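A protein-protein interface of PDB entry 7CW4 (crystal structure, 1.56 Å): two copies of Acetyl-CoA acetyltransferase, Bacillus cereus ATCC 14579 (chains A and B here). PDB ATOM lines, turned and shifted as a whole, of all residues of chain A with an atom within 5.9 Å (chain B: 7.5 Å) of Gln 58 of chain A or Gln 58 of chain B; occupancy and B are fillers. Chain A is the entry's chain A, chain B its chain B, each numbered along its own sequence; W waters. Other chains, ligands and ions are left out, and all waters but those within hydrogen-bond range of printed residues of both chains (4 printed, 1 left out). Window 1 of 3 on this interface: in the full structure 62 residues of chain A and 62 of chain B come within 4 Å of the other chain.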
ATOM      1  N   THR A  55      31.858  -1.015  -4.059  1.00  0.00           N
ATOM      2  CA  THR A  55      30.920  -1.987  -4.683  1.00  0.00           C
ATOM      3  C   THR A  55      29.524  -1.423  -4.495  1.00  0.00           C
ATOM      4  O   THR A  55      29.278  -0.772  -3.458  1.00  0.00           O
ATOM      5  CB  THR A  55      31.104  -3.396  -4.120  1.00  0.00           C
ATOM      6  OG1 THR A  55      30.312  -4.282  -4.897  1.00  0.00           O
ATOM      7  CG2 THR A  55      30.782  -3.535  -2.657  1.00  0.00           C
ATOM      8  N   VAL A  56      28.693  -1.536  -5.524  1.00  0.00           N
ATOM      9  CA  VAL A  56      27.379  -0.874  -5.488  1.00  0.00           C
ATOM     10  C   VAL A  56      26.271  -1.794  -4.983  1.00  0.00           C
ATOM     11  O   VAL A  56      25.449  -1.307  -4.213  1.00  0.00           O
ATOM     12  CB  VAL A  56      27.052  -0.344  -6.862  1.00  0.00           C
ATOM     13  CG1 VAL A  56      25.718   0.370  -6.849  1.00  0.00           C
ATOM     14  CG2 VAL A  56      28.140   0.580  -7.361  1.00  0.00           C
ATOM     15  N   ILE A  57      26.197  -3.034  -5.477  1.00  0.00           N
ATOM     16  CA  ILE A  57      25.066  -3.931  -5.102  1.00  0.00           C
ATOM     17  C   ILE A  57      25.546  -4.753  -3.904  1.00  0.00           C
ATOM     18  O   ILE A  57      25.931  -5.925  -4.036  1.00  0.00           O
ATOM     19  CB  ILE A  57      24.558  -4.777  -6.288  1.00  0.00           C
ATOM     20  CG1 ILE A  57      24.397  -3.939  -7.564  1.00  0.00           C
ATOM     21  CG2 ILE A  57      23.254  -5.464  -5.881  1.00  0.00           C
ATOM     22  CD1 ILE A  57      23.424  -2.809  -7.463  1.00  0.00           C
ATOM     23  N   GLN A  58      25.598  -4.088  -2.764  1.00  0.00           N
ATOM     24  CA  GLN A  58      26.098  -4.731  -1.521  1.00  0.00           C
ATOM     25  C   GLN A  58      25.089  -5.757  -1.003  1.00  0.00           C
ATOM     26  O   GLN A  58      25.513  -6.631  -0.228  1.00  0.00           O
ATOM     27  CB  GLN A  58      26.424  -3.668  -0.474  1.00  0.00           C
ATOM     28  CG  GLN A  58      27.553  -2.778  -0.938  1.00  0.00           C
ATOM     29  CD  GLN A  58      27.943  -1.713   0.050  1.00  0.00           C
ATOM     30  OE1 GLN A  58      27.665  -1.834   1.262  1.00  0.00           O
ATOM     31  NE2 GLN A  58      28.574  -0.672  -0.495  1.00  0.00           N
ATOM     32  N   GLY A  59      23.817  -5.612  -1.313  1.00  0.00           N
ATOM     33  CA  GLY A  59      22.824  -6.528  -0.766  1.00  0.00           C
ATOM     34  C   GLY A  59      23.148  -7.964  -1.073  1.00  0.00           C
ATOM     35  O   GLY A  59      23.295  -8.318  -2.267  1.00  0.00           O
ATOM     36  N   GLY A  60      23.299  -8.761  -0.001  1.00  0.00           N
ATOM     37  CA  GLY A  60      23.576 -10.191  -0.049  1.00  0.00           C
ATOM     38  C   GLY A  60      25.044 -10.518  -0.108  1.00  0.00           C
ATOM     39  O   GLY A  60      25.379 -11.708  -0.162  1.00  0.00           O
ATOM     40  N   GLN A  61      25.929  -9.517  -0.169  1.00  0.00           N
ATOM     41  CA  GLN A  61      27.373  -9.811  -0.197  1.00  0.00           C
ATOM     42  C   GLN A  61      27.897 -10.127   1.186  1.00  0.00           C
ATOM     43  O   GLN A  61      29.018 -10.635   1.223  1.00  0.00           O
ATOM     44  CB  GLN A  61      28.172  -8.664  -0.768  1.00  0.00           C
ATOM     45  CG  GLN A  61      27.935  -8.417  -2.260  1.00  0.00           C
ATOM     46  CD  GLN A  61      29.001  -7.544  -2.862  1.00  0.00           C
ATOM     47  OE1 GLN A  61      28.743  -6.557  -3.586  1.00  0.00           O
ATOM     48  NE2 GLN A  61      30.191  -7.996  -2.701  1.00  0.00           N
ATOM     49  N   GLY A  62      27.102  -9.936   2.246  1.00  0.00           N
ATOM     50  CA  GLY A  62      27.590 -10.163   3.621  1.00  0.00           C
ATOM     51  C   GLY A  62      28.298  -8.945   4.198  1.00  0.00           C
ATOM     52  O   GLY A  62      28.598  -7.928   3.520  1.00  0.00           O
ATOM     53  N   PRO A  65      31.931  -5.915   2.562  1.00  0.00           N
ATOM     54  CA  PRO A  65      32.571  -6.638   1.466  1.00  0.00           C
ATOM     55  C   PRO A  65      34.058  -6.307   1.205  1.00  0.00           C
ATOM     56  O   PRO A  65      34.814  -7.194   0.838  1.00  0.00           O
ATOM     57  CB  PRO A  65      31.697  -6.162   0.300  1.00  0.00           C
ATOM     58  CG  PRO A  65      30.327  -6.065   0.904  1.00  0.00           C
ATOM     59  CD  PRO A  65      30.608  -5.368   2.220  1.00  0.00           C
ATOM     60  N   THR A  83      34.088  -0.094   3.115  1.00  0.00           N
ATOM     61  CA  THR A  83      33.428  -0.233   1.801  1.00  0.00           C
ATOM     62  C   THR A  83      32.713   1.076   1.434  1.00  0.00           C
ATOM     63  O   THR A  83      31.985   1.662   2.266  1.00  0.00           O
ATOM     64  CB  THR A  83      32.465  -1.422   1.847  1.00  0.00           C
ATOM     65  OG1 THR A  83      33.132  -2.601   2.318  1.00  0.00           O
ATOM     66  CG2 THR A  83      31.918  -1.743   0.484  1.00  0.00           C
ATOM     67  N   VAL A  84      32.950   1.531   0.217  1.00  0.00           N
ATOM     68  CA  VAL A  84      32.397   2.820  -0.250  1.00  0.00           C
ATOM     69  C   VAL A  84      31.443   2.557  -1.421  1.00  0.00           C
ATOM     70  O   VAL A  84      31.601   1.579  -2.190  1.00  0.00           O
ATOM     71  CB  VAL A  84      33.513   3.819  -0.601  1.00  0.00           C
ATOM     72  CG1 VAL A  84      34.362   4.106   0.632  1.00  0.00           C
ATOM     73  CG2 VAL A  84      34.350   3.363  -1.744  1.00  0.00           C
ATOM     74  N   ASN A  85      30.442   3.426  -1.508  1.00  0.00           N
ATOM     75  CA  ASN A  85      29.396   3.398  -2.539  1.00  0.00           C
ATOM     76  C   ASN A  85      29.210   4.820  -3.050  1.00  0.00           C
ATOM     77  O   ASN A  85      28.684   5.689  -2.327  1.00  0.00           O
ATOM     78  CB  ASN A  85      28.115   2.776  -1.996  1.00  0.00           C
ATOM     79  CG  ASN A  85      26.996   2.675  -3.002  1.00  0.00           C
ATOM     80  OD1 ASN A  85      27.108   3.091  -4.135  1.00  0.00           O
ATOM     81  ND2 ASN A  85      25.904   2.067  -2.578  1.00  0.00           N
ATOM     82  N   GLU A 116      32.462  -5.737  -8.663  1.00  0.00           N
ATOM     83  CA  GLU A 116      31.025  -5.967  -8.855  1.00  0.00           C
ATOM     84  C   GLU A 116      30.863  -7.328  -9.516  1.00  0.00           C
ATOM     85  O   GLU A 116      31.599  -7.625 -10.452  1.00  0.00           O
ATOM     86  CB  GLU A 116      30.415  -4.873  -9.726  1.00  0.00           C
ATOM     87  CG  GLU A 116      28.931  -4.660  -9.417  1.00  0.00           C
ATOM     88  CD  GLU A 116      28.658  -3.871  -8.145  1.00  0.00           C
ATOM     89  OE1 GLU A 116      29.123  -2.732  -8.027  1.00  0.00           O
ATOM     90  OE2 GLU A 116      27.958  -4.405  -7.238  1.00  0.00           O
ATOM     91  N   LEU A 142      17.853  -6.741  -7.721  1.00  0.00           N
ATOM     92  CA  LEU A 142      18.586  -5.746  -6.929  1.00  0.00           C
ATOM     93  C   LEU A 142      19.572  -4.968  -7.803  1.00  0.00           C
ATOM     94  O   LEU A 142      19.820  -3.826  -7.465  1.00  0.00           O
ATOM     95  CB  LEU A 142      19.334  -6.399  -5.770  1.00  0.00           C
ATOM     96  CG  LEU A 142      19.626  -5.433  -4.646  1.00  0.00           C
ATOM     97  CD1 LEU A 142      18.360  -4.710  -4.188  1.00  0.00           C
ATOM     98  CD2 LEU A 142      20.307  -6.166  -3.509  1.00  0.00           C
ATOM     99  N   ASP A 146      18.912  -1.034  -6.954  1.00  0.00           N
ATOM    100  CA  ASP A 146      20.001  -0.332  -6.223  1.00  0.00           C
ATOM    101  C   ASP A 146      21.057   0.228  -7.175  1.00  0.00           C
ATOM    102  O   ASP A 146      21.836   1.085  -6.689  1.00  0.00           O
ATOM    103  CB  ASP A 146      20.607  -1.260  -5.160  1.00  0.00           C
ATOM    104  CG  ASP A 146      19.743  -1.484  -3.926  1.00  0.00           C
ATOM    105  OD1 ASP A 146      18.680  -0.776  -3.735  1.00  0.00           O
ATOM    106  OD2 ASP A 146      20.178  -2.348  -3.089  1.00  0.00           O
ATOM    107  N   PHE B  53      27.871   9.649   4.533  1.00  0.00           N
ATOM    108  CA  PHE B  53      26.850   9.027   5.401  1.00  0.00           C
ATOM    109  C   PHE B  53      27.009   7.530   5.423  1.00  0.00           C
ATOM    110  O   PHE B  53      27.131   6.915   4.349  1.00  0.00           O
ATOM    111  CB  PHE B  53      25.434   9.438   5.004  1.00  0.00           C
ATOM    112  CG  PHE B  53      24.667  10.060   6.134  1.00  0.00           C
ATOM    113  CD1 PHE B  53      25.038  11.274   6.691  1.00  0.00           C
ATOM    114  CD2 PHE B  53      23.584   9.394   6.690  1.00  0.00           C
ATOM    115  CE1 PHE B  53      24.345  11.782   7.786  1.00  0.00           C
ATOM    116  CE2 PHE B  53      22.885   9.938   7.751  1.00  0.00           C
ATOM    117  CZ  PHE B  53      23.239  11.141   8.276  1.00  0.00           C
ATOM    118  N   GLY B  54      26.899   6.975   6.631  1.00  0.00           N
ATOM    119  CA  GLY B  54      26.995   5.520   6.846  1.00  0.00           C
ATOM    120  C   GLY B  54      25.636   4.835   6.916  1.00  0.00           C
ATOM    121  O   GLY B  54      24.671   5.413   7.410  1.00  0.00           O
ATOM    122  N   THR B  55      25.554   3.625   6.369  1.00  0.00           N
ATOM    123  CA  THR B  55      24.399   2.726   6.542  1.00  0.00           C
ATOM    124  C   THR B  55      24.879   1.327   6.146  1.00  0.00           C
ATOM    125  O   THR B  55      25.648   1.182   5.179  1.00  0.00           O
ATOM    126  CB  THR B  55      23.184   3.217   5.757  1.00  0.00           C
ATOM    127  OG1 THR B  55      22.078   2.387   6.137  1.00  0.00           O
ATOM    128  CG2 THR B  55      23.344   3.198   4.251  1.00  0.00           C
ATOM    129  N   VAL B  56      24.472   0.323   6.883  1.00  0.00           N
ATOM    130  CA  VAL B  56      24.989  -1.047   6.677  1.00  0.00           C
ATOM    131  C   VAL B  56      24.077  -1.870   5.780  1.00  0.00           C
ATOM    132  O   VAL B  56      24.624  -2.591   4.926  1.00  0.00           O
ATOM    133  CB  VAL B  56      25.163  -1.736   8.020  1.00  0.00           C
ATOM    134  CG1 VAL B  56      25.773  -3.116   7.820  1.00  0.00           C
ATOM    135  CG2 VAL B  56      26.007  -0.915   8.987  1.00  0.00           C
ATOM    136  N   ILE B  57      22.743  -1.826   5.986  1.00  0.00           N
ATOM    137  CA  ILE B  57      21.864  -2.724   5.183  1.00  0.00           C
ATOM    138  C   ILE B  57      21.400  -1.915   3.973  1.00  0.00           C
ATOM    139  O   ILE B  57      20.288  -1.419   3.989  1.00  0.00           O
ATOM    140  CB  ILE B  57      20.723  -3.326   6.035  1.00  0.00           C
ATOM    141  CG1 ILE B  57      21.246  -3.848   7.375  1.00  0.00           C
ATOM    142  CG2 ILE B  57      20.007  -4.393   5.199  1.00  0.00           C
ATOM    143  CD1 ILE B  57      22.147  -5.023   7.254  1.00  0.00           C
ATOM    144  N   GLN B  58      22.308  -1.730   3.017  1.00  0.00           N
ATOM    145  CA  GLN B  58      22.010  -0.870   1.846  1.00  0.00           C
ATOM    146  C   GLN B  58      21.036  -1.579   0.926  1.00  0.00           C
ATOM    147  O   GLN B  58      20.404  -0.888   0.082  1.00  0.00           O
ATOM    148  CB  GLN B  58      23.316  -0.510   1.130  1.00  0.00           C
ATOM    149  CG  GLN B  58      24.172   0.388   1.993  1.00  0.00           C
ATOM    150  CD  GLN B  58      25.470   0.796   1.357  1.00  0.00           C
ATOM    151  OE1 GLN B  58      25.614   0.709   0.128  1.00  0.00           O
ATOM    152  NE2 GLN B  58      26.418   1.132   2.222  1.00  0.00           N
ATOM    153  N   GLY B  59      20.999  -2.906   0.926  1.00  0.00           N
ATOM    154  CA  GLY B  59      20.156  -3.631  -0.022  1.00  0.00           C
ATOM    155  C   GLY B  59      18.704  -3.166   0.068  1.00  0.00           C
ATOM    156  O   GLY B  59      18.098  -3.259   1.128  1.00  0.00           O
ATOM    157  N   GLY B  60      18.172  -2.746  -1.080  1.00  0.00           N
ATOM    158  CA  GLY B  60      16.800  -2.267  -1.271  1.00  0.00           C
ATOM    159  C   GLY B  60      16.619  -0.817  -0.895  1.00  0.00           C
ATOM    160  O   GLY B  60      15.480  -0.347  -1.060  1.00  0.00           O
ATOM    161  N   GLN B  61      17.664  -0.100  -0.463  1.00  0.00           N
ATOM    162  CA  GLN B  61      17.518   1.344  -0.146  1.00  0.00           C
ATOM    163  C   GLN B  61      17.577   2.216  -1.397  1.00  0.00           C
ATOM    164  O   GLN B  61      17.219   3.399  -1.288  1.00  0.00           O
ATOM    165  CB  GLN B  61      18.598   1.828   0.791  1.00  0.00           C
ATOM    166  CG  GLN B  61      18.438   1.258   2.185  1.00  0.00           C
ATOM    167  CD  GLN B  61      19.168   2.109   3.193  1.00  0.00           C
ATOM    168  OE1 GLN B  61      18.993   3.310   3.244  1.00  0.00           O
ATOM    169  NE2 GLN B  61      19.977   1.482   4.020  1.00  0.00           N
ATOM    170  N   GLY B  62      17.952   1.667  -2.542  1.00  0.00           N
ATOM    171  CA  GLY B  62      18.088   2.451  -3.785  1.00  0.00           C
ATOM    172  C   GLY B  62      19.489   3.011  -3.956  1.00  0.00           C
ATOM    173  O   GLY B  62      20.306   2.956  -3.048  1.00  0.00           O
ATOM    174  N   GLN B  63      19.751   3.614  -5.116  1.00  0.00           N
ATOM    175  CA  GLN B  63      21.072   4.201  -5.426  1.00  0.00           C
ATOM    176  C   GLN B  63      21.530   5.137  -4.289  1.00  0.00           C
ATOM    177  O   GLN B  63      20.726   5.979  -3.828  1.00  0.00           O
ATOM    178  CB  GLN B  63      21.048   5.051  -6.709  1.00  0.00           C
ATOM    179  CG  GLN B  63      21.098   4.247  -7.993  1.00  0.00           C
ATOM    180  CD  GLN B  63      21.164   5.183  -9.185  1.00  0.00           C
ATOM    181  OE1 GLN B  63      20.742   6.343  -9.125  1.00  0.00           O
ATOM    182  NE2 GLN B  63      21.543   4.620 -10.303  1.00  0.00           N
ATOM    183  N   ILE B  64      22.792   4.999  -3.925  1.00  0.00           N
ATOM    184  CA  ILE B  64      23.583   5.910  -3.050  1.00  0.00           C
ATOM    185  C   ILE B  64      22.708   6.537  -1.980  1.00  0.00           C
ATOM    186  O   ILE B  64      22.285   7.698  -2.024  1.00  0.00           O
ATOM    187  CB  ILE B  64      24.396   6.896  -3.900  1.00  0.00           C
ATOM    188  CG1 ILE B  64      25.395   7.652  -3.054  1.00  0.00           C
ATOM    189  CG2 ILE B  64      23.531   7.782  -4.799  1.00  0.00           C
ATOM    190  CD1 ILE B  64      26.261   8.530  -3.850  1.00  0.00           C
ATOM    191  N   PRO B  65      22.375   5.740  -0.931  1.00  0.00           N
ATOM    192  CA  PRO B  65      21.513   6.236   0.151  1.00  0.00           C
ATOM    193  C   PRO B  65      21.923   7.583   0.775  1.00  0.00           C
ATOM    194  O   PRO B  65      21.045   8.366   1.156  1.00  0.00           O
ATOM    195  CB  PRO B  65      21.559   5.076   1.168  1.00  0.00           C
ATOM    196  CG  PRO B  65      21.703   3.877   0.264  1.00  0.00           C
ATOM    197  CD  PRO B  65      22.700   4.314  -0.777  1.00  0.00           C
ATOM    198  N   SER B  66      23.211   7.887   0.830  1.00  0.00           N
ATOM    199  CA  SER B  66      23.677   9.170   1.374  1.00  0.00           C
ATOM    200  C   SER B  66      23.043  10.337   0.612  1.00  0.00           C
ATOM    201  O   SER B  66      22.726  11.358   1.221  1.00  0.00           O
ATOM    202  CB  SER B  66      25.201   9.258   1.379  1.00  0.00           C
ATOM    203  OG  SER B  66      25.749   9.175   0.088  1.00  0.00           O
ATOM    204  N   GLN B  68      20.147  10.302  -0.999  1.00  0.00           N
ATOM    205  CA  GLN B  68      18.717  10.350  -0.647  1.00  0.00           C
ATOM    206  C   GLN B  68      18.585  11.101   0.688  1.00  0.00           C
ATOM    207  O   GLN B  68      17.678  11.955   0.801  1.00  0.00           O
ATOM    208  CB  GLN B  68      18.151   8.958  -0.595  1.00  0.00           C
ATOM    209  CG  GLN B  68      18.167   8.244  -1.931  1.00  0.00           C
ATOM    210  CD  GLN B  68      17.612   6.874  -1.780  1.00  0.00           C
ATOM    211  OE1 GLN B  68      16.456   6.709  -1.357  1.00  0.00           O
ATOM    212  NE2 GLN B  68      18.455   5.877  -2.030  1.00  0.00           N
ATOM    213  N   THR B  83      28.344   7.062   0.204  1.00  0.00           N
ATOM    214  CA  THR B  83      27.825   6.215   1.275  1.00  0.00           C
ATOM    215  C   THR B  83      28.945   5.272   1.733  1.00  0.00           C
ATOM    216  O   THR B  83      29.575   4.628   0.891  1.00  0.00           O
ATOM    217  CB  THR B  83      26.579   5.468   0.815  1.00  0.00           C
ATOM    218  OG1 THR B  83      25.659   6.399   0.272  1.00  0.00           O
ATOM    219  CG2 THR B  83      25.892   4.707   1.924  1.00  0.00           C
ATOM    220  N   VAL B  84      29.127   5.173   3.040  1.00  0.00           N
ATOM    221  CA  VAL B  84      30.175   4.322   3.637  1.00  0.00           C
ATOM    222  C   VAL B  84      29.585   3.221   4.498  1.00  0.00           C
ATOM    223  O   VAL B  84      28.501   3.348   5.084  1.00  0.00           O
ATOM    224  CB  VAL B  84      31.180   5.178   4.392  1.00  0.00           C
ATOM    225  CG1 VAL B  84      31.834   6.199   3.486  1.00  0.00           C
ATOM    226  CG2 VAL B  84      30.598   5.833   5.601  1.00  0.00           C
ATOM    227  N   ASN B  85      30.324   2.122   4.503  1.00  0.00           N
ATOM    228  CA  ASN B  85      29.943   0.895   5.216  1.00  0.00           C
ATOM    229  C   ASN B  85      31.185   0.422   5.954  1.00  0.00           C
ATOM    230  O   ASN B  85      32.104  -0.111   5.325  1.00  0.00           O
ATOM    231  CB  ASN B  85      29.352  -0.142   4.251  1.00  0.00           C
ATOM    232  CG  ASN B  85      28.892  -1.408   4.940  1.00  0.00           C
ATOM    233  OD1 ASN B  85      29.091  -1.601   6.141  1.00  0.00           O
ATOM    234  ND2 ASN B  85      28.359  -2.305   4.162  1.00  0.00           N
ATOM    235  N   LYS B  86      31.166   0.570   7.272  1.00  0.00           N
ATOM    236  CA  LYS B  86      32.119  -0.114   8.168  1.00  0.00           C
ATOM    237  C   LYS B  86      31.267  -0.822   9.231  1.00  0.00           C
ATOM    238  O   LYS B  86      31.639  -0.745  10.423  1.00  0.00           O
ATOM    239  CB  LYS B  86      33.144   0.889   8.700  1.00  0.00           C
ATOM    240  CG  LYS B  86      34.408   0.251   9.267  1.00  0.00           C
ATOM    241  CD  LYS B  86      35.474   1.207   9.734  1.00  0.00           C
ATOM    242  CE  LYS B  86      36.635   0.435  10.337  1.00  0.00           C
ATOM    243  NZ  LYS B  86      37.752   1.333  10.752  1.00  0.00           N
ATOM    244  N   SER B  90      30.009   2.412  10.933  1.00  0.00           N
ATOM    245  CA  SER B  90      29.766   3.231   9.713  1.00  0.00           C
ATOM    246  C   SER B  90      29.594   4.709  10.067  1.00  0.00           C
ATOM    247  O   SER B  90      30.166   5.561   9.387  1.00  0.00           O
ATOM    248  CB  SER B  90      28.561   2.721   8.961  1.00  0.00           C
ATOM    249  OG  SER B  90      28.766   1.397   8.482  1.00  0.00           O
ATOM    250  N   MET B 115      22.685   6.253   9.413  1.00  0.00           N
ATOM    251  CA  MET B 115      21.234   5.965   9.467  1.00  0.00           C
ATOM    252  C   MET B 115      21.078   4.463   9.388  1.00  0.00           C
ATOM    253  O   MET B 115      21.877   3.793   8.716  1.00  0.00           O
ATOM    254  CB  MET B 115      20.494   6.631   8.309  1.00  0.00           C
ATOM    255  CG  MET B 115      21.109   6.254   6.986  1.00  0.00           C
ATOM    256  SD  MET B 115      20.554   7.435   5.719  1.00  0.00           S
ATOM    257  CE  MET B 115      21.512   6.860   4.320  1.00  0.00           C
ATOM    258  N   GLU B 116      19.964   3.959   9.914  1.00  0.00           N
ATOM    259  CA  GLU B 116      19.574   2.568   9.700  1.00  0.00           C
ATOM    260  C   GLU B 116      18.083   2.431   9.996  1.00  0.00           C
ATOM    261  O   GLU B 116      17.615   3.032  10.977  1.00  0.00           O
ATOM    262  CB  GLU B 116      20.372   1.611  10.598  1.00  0.00           C
ATOM    263  CG  GLU B 116      20.475   0.239   9.984  1.00  0.00           C
ATOM    264  CD  GLU B 116      21.531   0.108   8.898  1.00  0.00           C
ATOM    265  OE1 GLU B 116      22.727   0.431   9.149  1.00  0.00           O
ATOM    266  OE2 GLU B 116      21.153  -0.357   7.770  1.00  0.00           O
ATOM    267  N   SER B 121      14.497  -3.447   6.393  1.00  0.00           N
ATOM    268  CA  SER B 121      15.411  -4.263   5.568  1.00  0.00           C
ATOM    269  C   SER B 121      14.566  -5.316   4.853  1.00  0.00           C
ATOM    270  O   SER B 121      13.623  -5.878   5.411  1.00  0.00           O
ATOM    271  CB  SER B 121      16.487  -4.893   6.382  1.00  0.00           C
ATOM    272  OG  SER B 121      17.193  -3.875   7.091  1.00  0.00           O
ATOM    273  N   PRO B 122      14.875  -5.634   3.591  1.00  0.00           N
ATOM    274  CA  PRO B 122      14.155  -6.675   2.868  1.00  0.00           C
ATOM    275  C   PRO B 122      14.585  -8.092   3.231  1.00  0.00           C
ATOM    276  O   PRO B 122      15.507  -8.314   4.010  1.00  0.00           O
ATOM    277  CB  PRO B 122      14.500  -6.404   1.409  1.00  0.00           C
ATOM    278  CG  PRO B 122      15.921  -5.852   1.511  1.00  0.00           C
ATOM    279  CD  PRO B 122      15.948  -5.024   2.776  1.00  0.00           C
ATOM    280  N   ILE B 124      15.800 -11.558   0.914  1.00  0.00           N
ATOM    281  CA  ILE B 124      16.429 -11.827  -0.398  1.00  0.00           C
ATOM    282  C   ILE B 124      16.341 -13.300  -0.763  1.00  0.00           C
ATOM    283  O   ILE B 124      16.138 -14.182   0.075  1.00  0.00           O
ATOM    284  CB  ILE B 124      17.889 -11.307  -0.472  1.00  0.00           C
ATOM    285  CG1 ILE B 124      18.829 -12.219   0.299  1.00  0.00           C
ATOM    286  CG2 ILE B 124      17.983  -9.879   0.013  1.00  0.00           C
ATOM    287  CD1 ILE B 124      20.300 -11.851   0.004  1.00  0.00           C
ATOM    288  N   LEU B 142      17.790  -9.927   5.288  1.00  0.00           N
ATOM    289  CA  LEU B 142      19.037  -9.169   5.004  1.00  0.00           C
ATOM    290  C   LEU B 142      19.667  -8.548   6.261  1.00  0.00           C
ATOM    291  O   LEU B 142      20.931  -8.353   6.239  1.00  0.00           O
ATOM    292  CB  LEU B 142      18.772  -8.088   3.954  1.00  0.00           C
ATOM    293  CG  LEU B 142      19.995  -7.755   3.124  1.00  0.00           C
ATOM    294  CD1 LEU B 142      20.595  -9.009   2.496  1.00  0.00           C
ATOM    295  CD2 LEU B 142      19.637  -6.713   2.061  1.00  0.00           C
ATOM    296  N   ASP B 146      23.617  -9.516   6.070  1.00  0.00           N
ATOM    297  CA  ASP B 146      24.562  -8.398   5.785  1.00  0.00           C
ATOM    298  C   ASP B 146      24.993  -7.671   7.063  1.00  0.00           C
ATOM    299  O   ASP B 146      25.985  -6.904   6.968  1.00  0.00           O
ATOM    300  CB  ASP B 146      23.980  -7.466   4.731  1.00  0.00           C
ATOM    301  CG  ASP B 146      23.979  -8.059   3.310  1.00  0.00           C
ATOM    302  OD1 ASP B 146      24.600  -9.119   3.033  1.00  0.00           O
ATOM    303  OD2 ASP B 146      23.350  -7.414   2.422  1.00  0.00           O
HETATM  304  O   HOH W   1      23.335   1.520  -4.049  1.00  0.00           O
HETATM  305  O   HOH W   2      15.800  -0.072  -4.032  1.00  0.00           O
HETATM  306  O   HOH W   3      25.285  -2.950   2.413  1.00  0.00           O
HETATM  307  O   HOH W   4      24.543  -1.162  -1.739  1.00  0.00           O
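O of Thr 83 of chain A sits at hydrogen-bond distance from N of Asn 85 of chain B (2.8 Å). The backbone NH (N) of Gly 60 of chain B sits at hydrogen-bond distance from the side-chain carboxylate (OD2) of Asp 146 of chain A. The side-chain carboxylate (OD1) of Asp 146 of chain B is in hydrogen-bond range of the backbone NH (N) of Gly 62 of chain A. The backbone NH (N) of Gln 61 of chain A sits at hydrogen-bond distance from the side-chain carboxylate (OD1) of Asp 146 of chain B (3.5 Å). ND2 of Asn 85 of chain B lies within hydrogen-bond range of OE1 of Gln 58 of chain A. The side-chain carboxylate of Asp 146 of chain A sits close to the backbone carbonyl oxygen of Gln 58 of chain B (3.5 Å). OD1 of Asp 146 of chain A lies within hydrogen-bond range of N of Gln 61 of chain B (3.5 Å). The backbone carbonyl oxygen of Thr 83 of chain B is in hydrogen-bond range of the backbone NH of Asn 85 of chain A, 2.8 Å away. NE2 of Gln 58 of chain A is in hydrogen-bond range of OE1 of Gln 58 of chain B, 3.3 Å away. ND2 of Asn 85 of chain A is in hydrogen-bond range of OE1 of Gln 58 of chain B (3.0 Å). OD2 of Asp 146 of chain B sits at hydrogen-bond distance from N of Gly 60 of chain A. The side-chain carboxylate (OD1) of Asp 146 of chain A sits at hydrogen-bond distance from the backbone NH (N) of Gly 62 of chain B (2.8 Å).
NE2 of Gln 58 of chain B sits at hydrogen-bond distance from O of Thr 55 of chain B. OG1 of Thr 55 of chain A is in hydrogen-bond range of OE1 of Gln 61 of chain A (3.1 Å).
Of chain B, only Gln 58, Asn 85 and Asp 146 come within 4 Å of Gln 58 of chain A. Printed residues of chain B within 4 Å of Gly 59 of chain A: Asp 146. Of the printed residues of chain B, Gly 62 of chain A touches Asp 146 (2.7 Å). Gln 58 of chain B touches just these residues of chain A: Gln 58 (3.3 Å), Asn 85 (3.0 Å) and Asp 146 (3.5 Å). The nearest residue of chain B that does not touch Gln 58 of chain A is Val 56 of chain B (4.8 Å). The nearest residue of chain A that does not touch Gln 58 of chain B is Val 56 of chain A (4.8 Å). The nearest printed residue of chain A that does not touch Asp 146 of chain B is Leu 142 of chain A (6.8 Å).
Printed residues of chain A that touch a printed residue of chain B: Gln 58, Gly 59, Gly 60, Gln 61, Gly 62, Thr 83, Val 84, Asn 85, Leu 142 and Asp 146. Hydrophobic or aromatic side chains of chain A within 4 Å of the printed part of chain B: Leu 142. Hydrophobic or aromatic side chains of chain B within 4 Å of the printed part of chain A: Ile 64, Ile 124 and Leu 142.
Gly 60 of chain A touches Asp 146 of chain B, and with the chains exchanged Asp 146 of chain A touches Gly 60 of chain B. Thr 83 of chain A touches Val 84 of chain B, and with the chains exchanged Val 84 of chain A touches Thr 83 of chain B.
Water W2 lies within hydrogen-bond range of the side-chain carboxylate (OD1) of Asp 146 of chain A (3.0 Å), the backbone carbonyl oxygen (O) of Gly 60 of chain B (3.0 Å) and the backbone NH (N) of Gly 62 of chain B (3.1 Å).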
